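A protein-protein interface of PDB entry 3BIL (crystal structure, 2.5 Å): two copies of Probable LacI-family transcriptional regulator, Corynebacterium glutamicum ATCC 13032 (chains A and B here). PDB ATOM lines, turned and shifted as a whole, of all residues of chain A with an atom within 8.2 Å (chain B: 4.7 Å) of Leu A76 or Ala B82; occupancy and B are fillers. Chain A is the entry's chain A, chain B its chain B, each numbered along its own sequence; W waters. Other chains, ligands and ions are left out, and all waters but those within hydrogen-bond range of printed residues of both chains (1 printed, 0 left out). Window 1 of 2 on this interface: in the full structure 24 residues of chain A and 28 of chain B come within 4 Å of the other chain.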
ATOM      1  N   VAL A  71       0.574  22.933  10.075  1.00  0.00           N
ATOM      2  CA  VAL A  71       1.781  22.720  10.898  1.00  0.00           C
ATOM      3  C   VAL A  71       2.660  21.609  10.380  1.00  0.00           C
ATOM      4  O   VAL A  71       2.178  20.559   9.947  1.00  0.00           O
ATOM      5  CB  VAL A  71       1.511  22.638  12.432  1.00  0.00           C
ATOM      6  CG1 VAL A  71       0.106  22.305  12.717  1.00  0.00           C
ATOM      7  CG2 VAL A  71       2.442  21.678  13.120  1.00  0.00           C
ATOM      8  N   ILE A  72       3.956  21.894  10.399  1.00  0.00           N
ATOM      9  CA  ILE A  72       4.982  20.987   9.909  1.00  0.00           C
ATOM     10  C   ILE A  72       5.975  20.672  11.013  1.00  0.00           C
ATOM     11  O   ILE A  72       6.490  21.574  11.665  1.00  0.00           O
ATOM     12  CB  ILE A  72       5.771  21.599   8.760  1.00  0.00           C
ATOM     13  CG1 ILE A  72       4.825  22.005   7.632  1.00  0.00           C
ATOM     14  CG2 ILE A  72       6.826  20.607   8.264  1.00  0.00           C
ATOM     15  CD1 ILE A  72       5.435  22.995   6.647  1.00  0.00           C
ATOM     16  N   VAL A  73       6.261  19.387  11.186  1.00  0.00           N
ATOM     17  CA  VAL A  73       7.056  18.915  12.308  1.00  0.00           C
ATOM     18  C   VAL A  73       8.000  17.807  11.827  1.00  0.00           C
ATOM     19  O   VAL A  73       7.677  17.116  10.846  1.00  0.00           O
ATOM     20  CB  VAL A  73       6.104  18.488  13.411  1.00  0.00           C
ATOM     21  CG1 VAL A  73       5.843  16.976  13.399  1.00  0.00           C
ATOM     22  CG2 VAL A  73       6.600  18.996  14.728  1.00  0.00           C
ATOM     23  N   PRO A  74       9.203  17.681  12.426  1.00  0.00           N
ATOM     24  CA  PRO A  74      10.147  16.701  11.875  1.00  0.00           C
ATOM     25  C   PRO A  74       9.809  15.246  12.155  1.00  0.00           C
ATOM     26  O   PRO A  74      10.324  14.335  11.498  1.00  0.00           O
ATOM     27  CB  PRO A  74      11.445  17.047  12.587  1.00  0.00           C
ATOM     28  CG  PRO A  74      11.035  17.624  13.840  1.00  0.00           C
ATOM     29  CD  PRO A  74       9.815  18.431  13.528  1.00  0.00           C
ATOM     30  N   SER A  75       8.962  15.015  13.136  1.00  0.00           N
ATOM     31  CA  SER A  75       8.714  13.649  13.578  1.00  0.00           C
ATOM     32  C   SER A  75       7.440  13.651  14.408  1.00  0.00           C
ATOM     33  O   SER A  75       7.100  14.668  15.027  1.00  0.00           O
ATOM     34  CB  SER A  75       9.906  13.162  14.421  1.00  0.00           C
ATOM     35  OG  SER A  75       9.571  12.064  15.247  1.00  0.00           O
ATOM     36  N   LEU A  76       6.756  12.512  14.399  1.00  0.00           N
ATOM     37  CA  LEU A  76       5.530  12.319  15.179  1.00  0.00           C
ATOM     38  C   LEU A  76       5.692  11.206  16.215  1.00  0.00           C
ATOM     39  O   LEU A  76       5.007  11.211  17.239  1.00  0.00           O
ATOM     40  CB  LEU A  76       4.293  12.099  14.267  1.00  0.00           C
ATOM     41  CG  LEU A  76       3.825  13.317  13.433  1.00  0.00           C
ATOM     42  CD1 LEU A  76       2.809  12.923  12.351  1.00  0.00           C
ATOM     43  CD2 LEU A  76       3.243  14.416  14.310  1.00  0.00           C
ATOM     44  N   ILE A  77       6.601  10.266  15.961  1.00  0.00           N
ATOM     45  CA  ILE A  77       6.988   9.314  17.006  1.00  0.00           C
ATOM     46  C   ILE A  77       7.804   9.990  18.113  1.00  0.00           C
ATOM     47  O   ILE A  77       7.913   9.459  19.207  1.00  0.00           O
ATOM     48  CB  ILE A  77       7.681   7.999  16.479  1.00  0.00           C
ATOM     49  CG1 ILE A  77       9.017   8.273  15.795  1.00  0.00           C
ATOM     50  CG2 ILE A  77       6.758   7.208  15.533  1.00  0.00           C
ATOM     51  CD1 ILE A  77       9.911   7.008  15.665  1.00  0.00           C
ATOM     52  N   ASN A  78       8.385  11.156  17.839  1.00  0.00           N
ATOM     53  CA  ASN A  78       8.842  11.995  18.932  1.00  0.00           C
ATOM     54  C   ASN A  78       7.632  12.491  19.751  1.00  0.00           C
ATOM     55  O   ASN A  78       6.720  13.179  19.240  1.00  0.00           O
ATOM     56  CB  ASN A  78       9.698  13.160  18.448  1.00  0.00           C
ATOM     57  CG  ASN A  78      10.575  13.749  19.559  1.00  0.00           C
ATOM     58  OD1 ASN A  78      10.102  14.061  20.647  1.00  0.00           O
ATOM     59  ND2 ASN A  78      11.858  13.910  19.273  1.00  0.00           N
ATOM     60  N   HIS A  79       7.617  12.107  21.020  1.00  0.00           N
ATOM     61  CA  HIS A  79       6.496  12.399  21.854  1.00  0.00           C
ATOM     62  C   HIS A  79       6.442  13.892  22.077  1.00  0.00           C
ATOM     63  O   HIS A  79       5.363  14.451  22.263  1.00  0.00           O
ATOM     64  CB  HIS A  79       6.601  11.649  23.170  1.00  0.00           C
ATOM     65  CG  HIS A  79       5.687  12.166  24.235  1.00  0.00           C
ATOM     66  ND1 HIS A  79       6.087  13.099  25.172  1.00  0.00           N
ATOM     67  CD2 HIS A  79       4.393  11.880  24.515  1.00  0.00           C
ATOM     68  CE1 HIS A  79       5.081  13.356  25.990  1.00  0.00           C
ATOM     69  NE2 HIS A  79       4.038  12.636  25.608  1.00  0.00           N
ATOM     70  N   TYR A  80       7.593  14.550  22.029  1.00  0.00           N
ATOM     71  CA  TYR A  80       7.624  15.993  22.211  1.00  0.00           C
ATOM     72  C   TYR A  80       6.938  16.748  21.076  1.00  0.00           C
ATOM     73  O   TYR A  80       6.145  17.654  21.307  1.00  0.00           O
ATOM     74  CB  TYR A  80       9.053  16.458  22.336  1.00  0.00           C
ATOM     75  CG  TYR A  80       9.218  17.956  22.312  1.00  0.00           C
ATOM     76  CD1 TYR A  80       9.118  18.717  23.481  1.00  0.00           C
ATOM     77  CD2 TYR A  80       9.501  18.610  21.115  1.00  0.00           C
ATOM     78  CE1 TYR A  80       9.296  20.068  23.461  1.00  0.00           C
ATOM     79  CE2 TYR A  80       9.666  19.968  21.081  1.00  0.00           C
ATOM     80  CZ  TYR A  80       9.570  20.689  22.259  1.00  0.00           C
ATOM     81  OH  TYR A  80       9.768  22.038  22.192  1.00  0.00           O
ATOM     82  N   PHE A  81       7.261  16.379  19.849  1.00  0.00           N
ATOM     83  CA  PHE A  81       6.655  16.987  18.717  1.00  0.00           C
ATOM     84  C   PHE A  81       5.176  16.578  18.538  1.00  0.00           C
ATOM     85  O   PHE A  81       4.406  17.314  17.906  1.00  0.00           O
ATOM     86  CB  PHE A  81       7.475  16.648  17.479  1.00  0.00           C
ATOM     87  CG  PHE A  81       8.780  17.376  17.399  1.00  0.00           C
ATOM     88  CD1 PHE A  81       8.825  18.769  17.450  1.00  0.00           C
ATOM     89  CD2 PHE A  81       9.967  16.676  17.252  1.00  0.00           C
ATOM     90  CE1 PHE A  81      10.056  19.457  17.365  1.00  0.00           C
ATOM     91  CE2 PHE A  81      11.197  17.344  17.148  1.00  0.00           C
ATOM     92  CZ  PHE A  81      11.257  18.739  17.217  1.00  0.00           C
ATOM     93  N   ALA A  82       4.779  15.411  19.066  1.00  0.00           N
ATOM     94  CA  ALA A  82       3.360  15.027  19.034  1.00  0.00           C
ATOM     95  C   ALA A  82       2.600  15.809  20.125  1.00  0.00           C
ATOM     96  O   ALA A  82       1.447  16.229  19.935  1.00  0.00           O
ATOM     97  CB  ALA A  82       3.195  13.525  19.196  1.00  0.00           C
ATOM     98  N   ALA A  83       3.260  16.033  21.260  1.00  0.00           N
ATOM     99  CA  ALA A  83       2.707  16.918  22.293  1.00  0.00           C
ATOM    100  C   ALA A  83       2.530  18.333  21.757  1.00  0.00           C
ATOM    101  O   ALA A  83       1.487  18.916  21.912  1.00  0.00           O
ATOM    102  CB  ALA A  83       3.577  16.906  23.562  1.00  0.00           C
ATOM    103  N   MET A  84       3.549  18.869  21.101  1.00  0.00           N
ATOM    104  CA  MET A  84       3.477  20.208  20.567  1.00  0.00           C
ATOM    105  C   MET A  84       2.288  20.386  19.600  1.00  0.00           C
ATOM    106  O   MET A  84       1.605  21.411  19.656  1.00  0.00           O
ATOM    107  CB  MET A  84       4.781  20.586  19.887  1.00  0.00           C
ATOM    108  CG  MET A  84       4.874  22.094  19.538  1.00  0.00           C
ATOM    109  SD  MET A  84       6.296  22.257  18.491  1.00  0.00           S
ATOM    110  CE  MET A  84       7.559  22.318  19.765  1.00  0.00           C
ATOM    111  N   VAL A  85       2.045  19.418  18.716  1.00  0.00           N
ATOM    112  CA  VAL A  85       0.962  19.572  17.740  1.00  0.00           C
ATOM    113  C   VAL A  85      -0.407  19.360  18.376  1.00  0.00           C
ATOM    114  O   VAL A  85      -1.353  20.035  18.016  1.00  0.00           O
ATOM    115  CB  VAL A  85       1.141  18.735  16.438  1.00  0.00           C
ATOM    116  CG1 VAL A  85       2.496  19.022  15.801  1.00  0.00           C
ATOM    117  CG2 VAL A  85       0.948  17.238  16.690  1.00  0.00           C
ATOM    118  N   THR A  86      -0.515  18.452  19.335  1.00  0.00           N
ATOM    119  CA  THR A  86      -1.747  18.319  20.069  1.00  0.00           C
ATOM    120  C   THR A  86      -2.076  19.686  20.688  1.00  0.00           C
ATOM    121  O   THR A  86      -3.188  20.169  20.545  1.00  0.00           O
ATOM    122  CB  THR A  86      -1.625  17.258  21.171  1.00  0.00           C
ATOM    123  OG1 THR A  86      -1.189  16.031  20.597  1.00  0.00           O
ATOM    124  CG2 THR A  86      -2.944  17.026  21.883  1.00  0.00           C
ATOM    125  N   ILE A 101      -1.654  18.724   9.718  1.00  0.00           N
ATOM    126  CA  ILE A 101      -0.307  18.456  10.202  1.00  0.00           C
ATOM    127  C   ILE A 101       0.528  17.833   9.120  1.00  0.00           C
ATOM    128  O   ILE A 101       0.031  17.018   8.353  1.00  0.00           O
ATOM    129  CB  ILE A 101      -0.311  17.490  11.442  1.00  0.00           C
ATOM    130  CG1 ILE A 101      -1.209  18.026  12.565  1.00  0.00           C
ATOM    131  CG2 ILE A 101       1.114  17.245  11.977  1.00  0.00           C
ATOM    132  CD1 ILE A 101      -2.424  17.201  12.782  1.00  0.00           C
ATOM    133  N   THR A 102       1.807  18.188   9.062  1.00  0.00           N
ATOM    134  CA  THR A 102       2.740  17.389   8.254  1.00  0.00           C
ATOM    135  C   THR A 102       4.043  16.995   8.960  1.00  0.00           C
ATOM    136  O   THR A 102       4.483  17.631   9.911  1.00  0.00           O
ATOM    137  CB  THR A 102       3.101  18.009   6.854  1.00  0.00           C
ATOM    138  OG1 THR A 102       4.356  18.705   6.936  1.00  0.00           O
ATOM    139  CG2 THR A 102       1.997  18.928   6.297  1.00  0.00           C
ATOM    140  N   ASN A 103       4.677  15.966   8.417  1.00  0.00           N
ATOM    141  CA  ASN A 103       5.779  15.310   9.037  1.00  0.00           C
ATOM    142  C   ASN A 103       6.894  15.227   8.022  1.00  0.00           C
ATOM    143  O   ASN A 103       6.749  14.561   7.012  1.00  0.00           O
ATOM    144  CB  ASN A 103       5.323  13.922   9.435  1.00  0.00           C
ATOM    145  CG  ASN A 103       6.415  13.111  10.093  1.00  0.00           C
ATOM    146  OD1 ASN A 103       7.548  13.562  10.251  1.00  0.00           O
ATOM    147  ND2 ASN A 103       6.074  11.900  10.495  1.00  0.00           N
ATOM    148  N   SER A 104       8.014  15.895   8.291  1.00  0.00           N
ATOM    149  CA  SER A 104       9.108  15.999   7.317  1.00  0.00           C
ATOM    150  C   SER A 104      10.160  14.900   7.381  1.00  0.00           C
ATOM    151  O   SER A 104      11.038  14.846   6.513  1.00  0.00           O
ATOM    152  CB  SER A 104       9.794  17.357   7.426  1.00  0.00           C
ATOM    153  OG  SER A 104      10.659  17.447   8.551  1.00  0.00           O
ATOM    154  N   ASN A 105      10.070  14.018   8.384  1.00  0.00           N
ATOM    155  CA  ASN A 105      11.126  13.015   8.672  1.00  0.00           C
ATOM    156  C   ASN A 105      12.554  13.522   8.697  1.00  0.00           C
ATOM    157  O   ASN A 105      13.472  12.762   8.395  1.00  0.00           O
ATOM    158  CB  ASN A 105      11.062  11.828   7.727  1.00  0.00           C
ATOM    159  CG  ASN A 105       9.766  11.133   7.809  1.00  0.00           C
ATOM    160  OD1 ASN A 105       8.940  11.249   6.903  1.00  0.00           O
ATOM    161  ND2 ASN A 105       9.525  10.449   8.929  1.00  0.00           N
ATOM    162  N   MET A 251      14.950  11.471  22.100  1.00  0.00           N
ATOM    163  CA  MET A 251      15.452  10.245  21.497  1.00  0.00           C
ATOM    164  C   MET A 251      16.766   9.794  22.132  1.00  0.00           C
ATOM    165  O   MET A 251      16.947   8.595  22.401  1.00  0.00           O
ATOM    166  CB  MET A 251      15.487  10.311  19.956  1.00  0.00           C
ATOM    167  CG  MET A 251      14.057  10.566  19.285  1.00  0.00           C
ATOM    168  SD  MET A 251      12.594   9.495  19.657  1.00  0.00           S
ATOM    169  CE  MET A 251      11.638  10.359  20.911  1.00  0.00           C
ATOM    170  N   LEU B  76      -2.365  11.595  18.394  1.00  0.00           N
ATOM    171  CA  LEU B  76      -0.957  11.573  17.995  1.00  0.00           C
ATOM    172  C   LEU B  76      -0.030  11.412  19.193  1.00  0.00           C
ATOM    173  O   LEU B  76       1.073  10.881  19.032  1.00  0.00           O
ATOM    174  CB  LEU B  76      -0.559  12.813  17.175  1.00  0.00           C
ATOM    175  CG  LEU B  76      -1.162  13.015  15.770  1.00  0.00           C
ATOM    176  CD1 LEU B  76      -0.869  14.422  15.307  1.00  0.00           C
ATOM    177  CD2 LEU B  76      -0.607  12.053  14.752  1.00  0.00           C
ATOM    178  N   ASN B  78      -0.790   9.298  21.287  1.00  0.00           N
ATOM    179  CA  ASN B  78      -0.806   7.842  21.178  1.00  0.00           C
ATOM    180  C   ASN B  78       0.315   7.312  20.236  1.00  0.00           C
ATOM    181  O   ASN B  78       0.334   7.567  19.009  1.00  0.00           O
ATOM    182  CB  ASN B  78      -2.183   7.355  20.720  1.00  0.00           C
ATOM    183  CG  ASN B  78      -2.397   5.833  20.935  1.00  0.00           C
ATOM    184  OD1 ASN B  78      -1.547   5.012  20.609  1.00  0.00           O
ATOM    185  ND2 ASN B  78      -3.564   5.472  21.450  1.00  0.00           N
ATOM    186  N   HIS B  79       1.256   6.580  20.834  1.00  0.00           N
ATOM    187  CA  HIS B  79       2.453   6.181  20.123  1.00  0.00           C
ATOM    188  C   HIS B  79       2.053   5.294  18.973  1.00  0.00           C
ATOM    189  O   HIS B  79       2.655   5.356  17.904  1.00  0.00           O
ATOM    190  CB  HIS B  79       3.468   5.478  21.042  1.00  0.00           C
ATOM    191  CG  HIS B  79       4.636   4.896  20.306  1.00  0.00           C
ATOM    192  ND1 HIS B  79       4.684   3.574  19.905  1.00  0.00           N
ATOM    193  CD2 HIS B  79       5.784   5.466  19.861  1.00  0.00           C
ATOM    194  CE1 HIS B  79       5.821   3.350  19.270  1.00  0.00           C
ATOM    195  NE2 HIS B  79       6.503   4.484  19.219  1.00  0.00           N
ATOM    196  N   TYR B  80       1.034   4.474  19.194  1.00  0.00           N
ATOM    197  CA  TYR B  80       0.554   3.561  18.176  1.00  0.00           C
ATOM    198  C   TYR B  80       0.036   4.292  16.910  1.00  0.00           C
ATOM    199  O   TYR B  80       0.336   3.901  15.784  1.00  0.00           O
ATOM    200  CB  TYR B  80      -0.520   2.661  18.774  1.00  0.00           C
ATOM    201  CG  TYR B  80      -1.238   1.812  17.759  1.00  0.00           C
ATOM    202  CD1 TYR B  80      -0.715   0.562  17.335  1.00  0.00           C
ATOM    203  CD2 TYR B  80      -2.442   2.253  17.211  1.00  0.00           C
ATOM    204  CE1 TYR B  80      -1.375  -0.202  16.409  1.00  0.00           C
ATOM    205  CE2 TYR B  80      -3.115   1.496  16.284  1.00  0.00           C
ATOM    206  CZ  TYR B  80      -2.584   0.276  15.880  1.00  0.00           C
ATOM    207  OH  TYR B  80      -3.316  -0.436  14.944  1.00  0.00           O
ATOM    208  N   PHE B  81      -0.719   5.366  17.090  1.00  0.00           N
ATOM    209  CA  PHE B  81      -1.211   6.105  15.945  1.00  0.00           C
ATOM    210  C   PHE B  81      -0.145   7.001  15.319  1.00  0.00           C
ATOM    211  O   PHE B  81      -0.254   7.347  14.152  1.00  0.00           O
ATOM    212  CB  PHE B  81      -2.448   6.905  16.343  1.00  0.00           C
ATOM    213  CG  PHE B  81      -3.654   6.053  16.602  1.00  0.00           C
ATOM    214  CD1 PHE B  81      -4.183   5.235  15.582  1.00  0.00           C
ATOM    215  CD2 PHE B  81      -4.273   6.076  17.847  1.00  0.00           C
ATOM    216  CE1 PHE B  81      -5.325   4.432  15.793  1.00  0.00           C
ATOM    217  CE2 PHE B  81      -5.419   5.275  18.106  1.00  0.00           C
ATOM    218  CZ  PHE B  81      -5.958   4.439  17.073  1.00  0.00           C
ATOM    219  N   ALA B  82       0.874   7.382  16.097  1.00  0.00           N
ATOM    220  CA  ALA B  82       1.995   8.147  15.557  1.00  0.00           C
ATOM    221  C   ALA B  82       2.863   7.228  14.697  1.00  0.00           C
ATOM    222  O   ALA B  82       3.327   7.620  13.629  1.00  0.00           O
ATOM    223  CB  ALA B  82       2.820   8.790  16.690  1.00  0.00           C
ATOM    224  N   ALA B  83       3.063   5.993  15.158  1.00  0.00           N
ATOM    225  CA  ALA B  83       3.734   4.953  14.372  1.00  0.00           C
ATOM    226  C   ALA B  83       2.934   4.596  13.137  1.00  0.00           C
ATOM    227  O   ALA B  83       3.507   4.457  12.073  1.00  0.00           O
ATOM    228  CB  ALA B  83       3.988   3.710  15.216  1.00  0.00           C
ATOM    229  N   MET B  84       1.611   4.457  13.269  1.00  0.00           N
ATOM    230  CA  MET B  84       0.803   4.107  12.117  1.00  0.00           C
ATOM    231  C   MET B  84       0.972   5.151  11.022  1.00  0.00           C
ATOM    232  O   MET B  84       1.215   4.788   9.871  1.00  0.00           O
ATOM    233  CB  MET B  84      -0.670   3.927  12.451  1.00  0.00           C
ATOM    234  CG  MET B  84      -1.480   3.323  11.282  1.00  0.00           C
ATOM    235  SD  MET B  84      -3.182   3.446  11.752  1.00  0.00           S
ATOM    236  CE  MET B  84      -3.173   2.209  13.049  1.00  0.00           C
ATOM    237  N   VAL B  85       0.885   6.436  11.370  1.00  0.00           N
ATOM    238  CA  VAL B  85       0.928   7.478  10.339  1.00  0.00           C
ATOM    239  C   VAL B  85       2.322   7.692   9.767  1.00  0.00           C
ATOM    240  O   VAL B  85       2.443   8.140   8.637  1.00  0.00           O
ATOM    241  CB  VAL B  85       0.301   8.822  10.762  1.00  0.00           C
ATOM    242  CG1 VAL B  85      -1.120   8.603  11.277  1.00  0.00           C
ATOM    243  CG2 VAL B  85       1.168   9.541  11.799  1.00  0.00           C
ATOM    244  N   THR B  86       3.359   7.385  10.537  1.00  0.00           N
ATOM    245  CA  THR B  86       4.716   7.496  10.043  1.00  0.00           C
ATOM    246  C   THR B  86       4.885   6.423   8.958  1.00  0.00           C
ATOM    247  O   THR B  86       5.412   6.706   7.879  1.00  0.00           O
ATOM    248  CB  THR B  86       5.733   7.249  11.176  1.00  0.00           C
ATOM    249  OG1 THR B  86       5.535   8.196  12.225  1.00  0.00           O
ATOM    250  CG2 THR B  86       7.163   7.323  10.690  1.00  0.00           C
ATOM    251  N   ILE B 101      -1.732  14.977   7.422  1.00  0.00           N
ATOM    252  CA  ILE B 101      -2.242  14.220   8.548  1.00  0.00           C
ATOM    253  C   ILE B 101      -3.192  15.095   9.307  1.00  0.00           C
ATOM    254  O   ILE B 101      -2.915  16.289   9.478  1.00  0.00           O
ATOM    255  CB  ILE B 101      -1.106  13.775   9.524  1.00  0.00           C
ATOM    256  CG1 ILE B 101      -0.141  12.788   8.857  1.00  0.00           C
ATOM    257  CG2 ILE B 101      -1.689  13.204  10.819  1.00  0.00           C
ATOM    258  CD1 ILE B 101       1.198  13.385   8.587  1.00  0.00           C
HETATM  259  O   HOH W   1       3.761  10.164  19.629  1.00  0.00           O
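Leu A76 touches Ala B82, and with the chains exchanged Ala A82 touches Leu B76. Leu A76 touches Val B85, and with the chains exchanged Val A85 touches Leu B76. Ile B101 touches its own counterpart, Ile A101. 11 positions are printed for both chains. Of the 8 pairs that touch across the chains among the printed residues, 5 have their exchanged pair printed and touching as well.
The backbone NH of Ile A101 lies within hydrogen-bond range of the backbone carbonyl oxygen of Ile B101.
Water W1 bridges the backbone carbonyl oxygen (O) of Leu B76 (2.8 Å) and the backbone carbonyl oxygen (O) of Leu A76 (2.9 Å).
Of the 11 printed residues of chain B, 6 touch a printed residue of chain A. Printed residues of chain B that touch a printed residue of chain A: Leu B76, Ala B82, Ala B83, Val B85, Thr B86 and Ile B101. Of the 22 printed residues of chain A, 5 touch a printed residue of chain B. Printed residues of chain A that touch a printed residue of chain B: Leu A76, Ile A77, Ala A82, Val A85 and Ile A101. Hydrophobic or aromatic side chains of chain A that line the printed part of chain B: Leu A76, Ile A77, Ala A82, Val A85 and Ile A101. Along chain A the printed residues that touch a printed residue of chain B span positions 76 to 101. Among the printed residues, 8 pairs touch across the chains. Among the printed residues, no Asp or Glu carboxylate lies within 4 Å of a Lys or Arg side-chain nitrogen of the other chain.
The backbone carbonyl oxygen of Ala A82 is in hydrogen-bond range of the side-chain hydroxyl of Thr A86 (2.7 Å). O of Ala B82 sits at hydrogen-bond distance from OG1 of Thr B86 (2.7 Å).
Printed residues of chain B within 4 Å of Leu A76: Ala B82 (3.3 Å) and Val B85 (3.8 Å). Of chain A, only Leu A76 (3.3 Å) and Ile A77 (3.9 Å) come within 4 Å of Ala B82. Of chain A, only Ile A77 comes within 4 Å of Ala B83. Printed residues of chain B within 4 Å of Ile A77: Ala B82 (3.9 Å), Ala B83 (3.9 Å) and Thr B86 (3.7 Å). Printed residues of chain B within 4 Å of Ile A101: Ile B101. Of the printed residues of chain B, Ala A82 touches Leu B76 (3.4 Å). Printed residues of chain A within 4 Å of Leu B76: Ala A82 and Val A85. Printed residues of chain A within 4 Å of Thr B86: Ile A77. Met B84 touches none of the printed residues of chain A. The nearest residue of chain B that does not touch Leu A76 is Ile B101 (4.1 Å). The nearest residue of chain A that does not touch Ala B82 is Ala A82 (5.4 Å).
Leu A76 touches Ala B82 (O to CB, 3.3 Å). Leu A76 touches Val B85 (CD1 to CG2, 3.8 Å). O of Ala B82 touches CG2 of Ile A77 (3.9 Å). N of Ala B83 touches CG2 of Ile A77, 3.9 Å away. Ile A77 touches Thr B86 (CG2 to OG1, 3.7 Å). Ala A82 touches Leu B76. Val A85 touches Leu B76 (CG2 to CD1, 3.6 Å).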
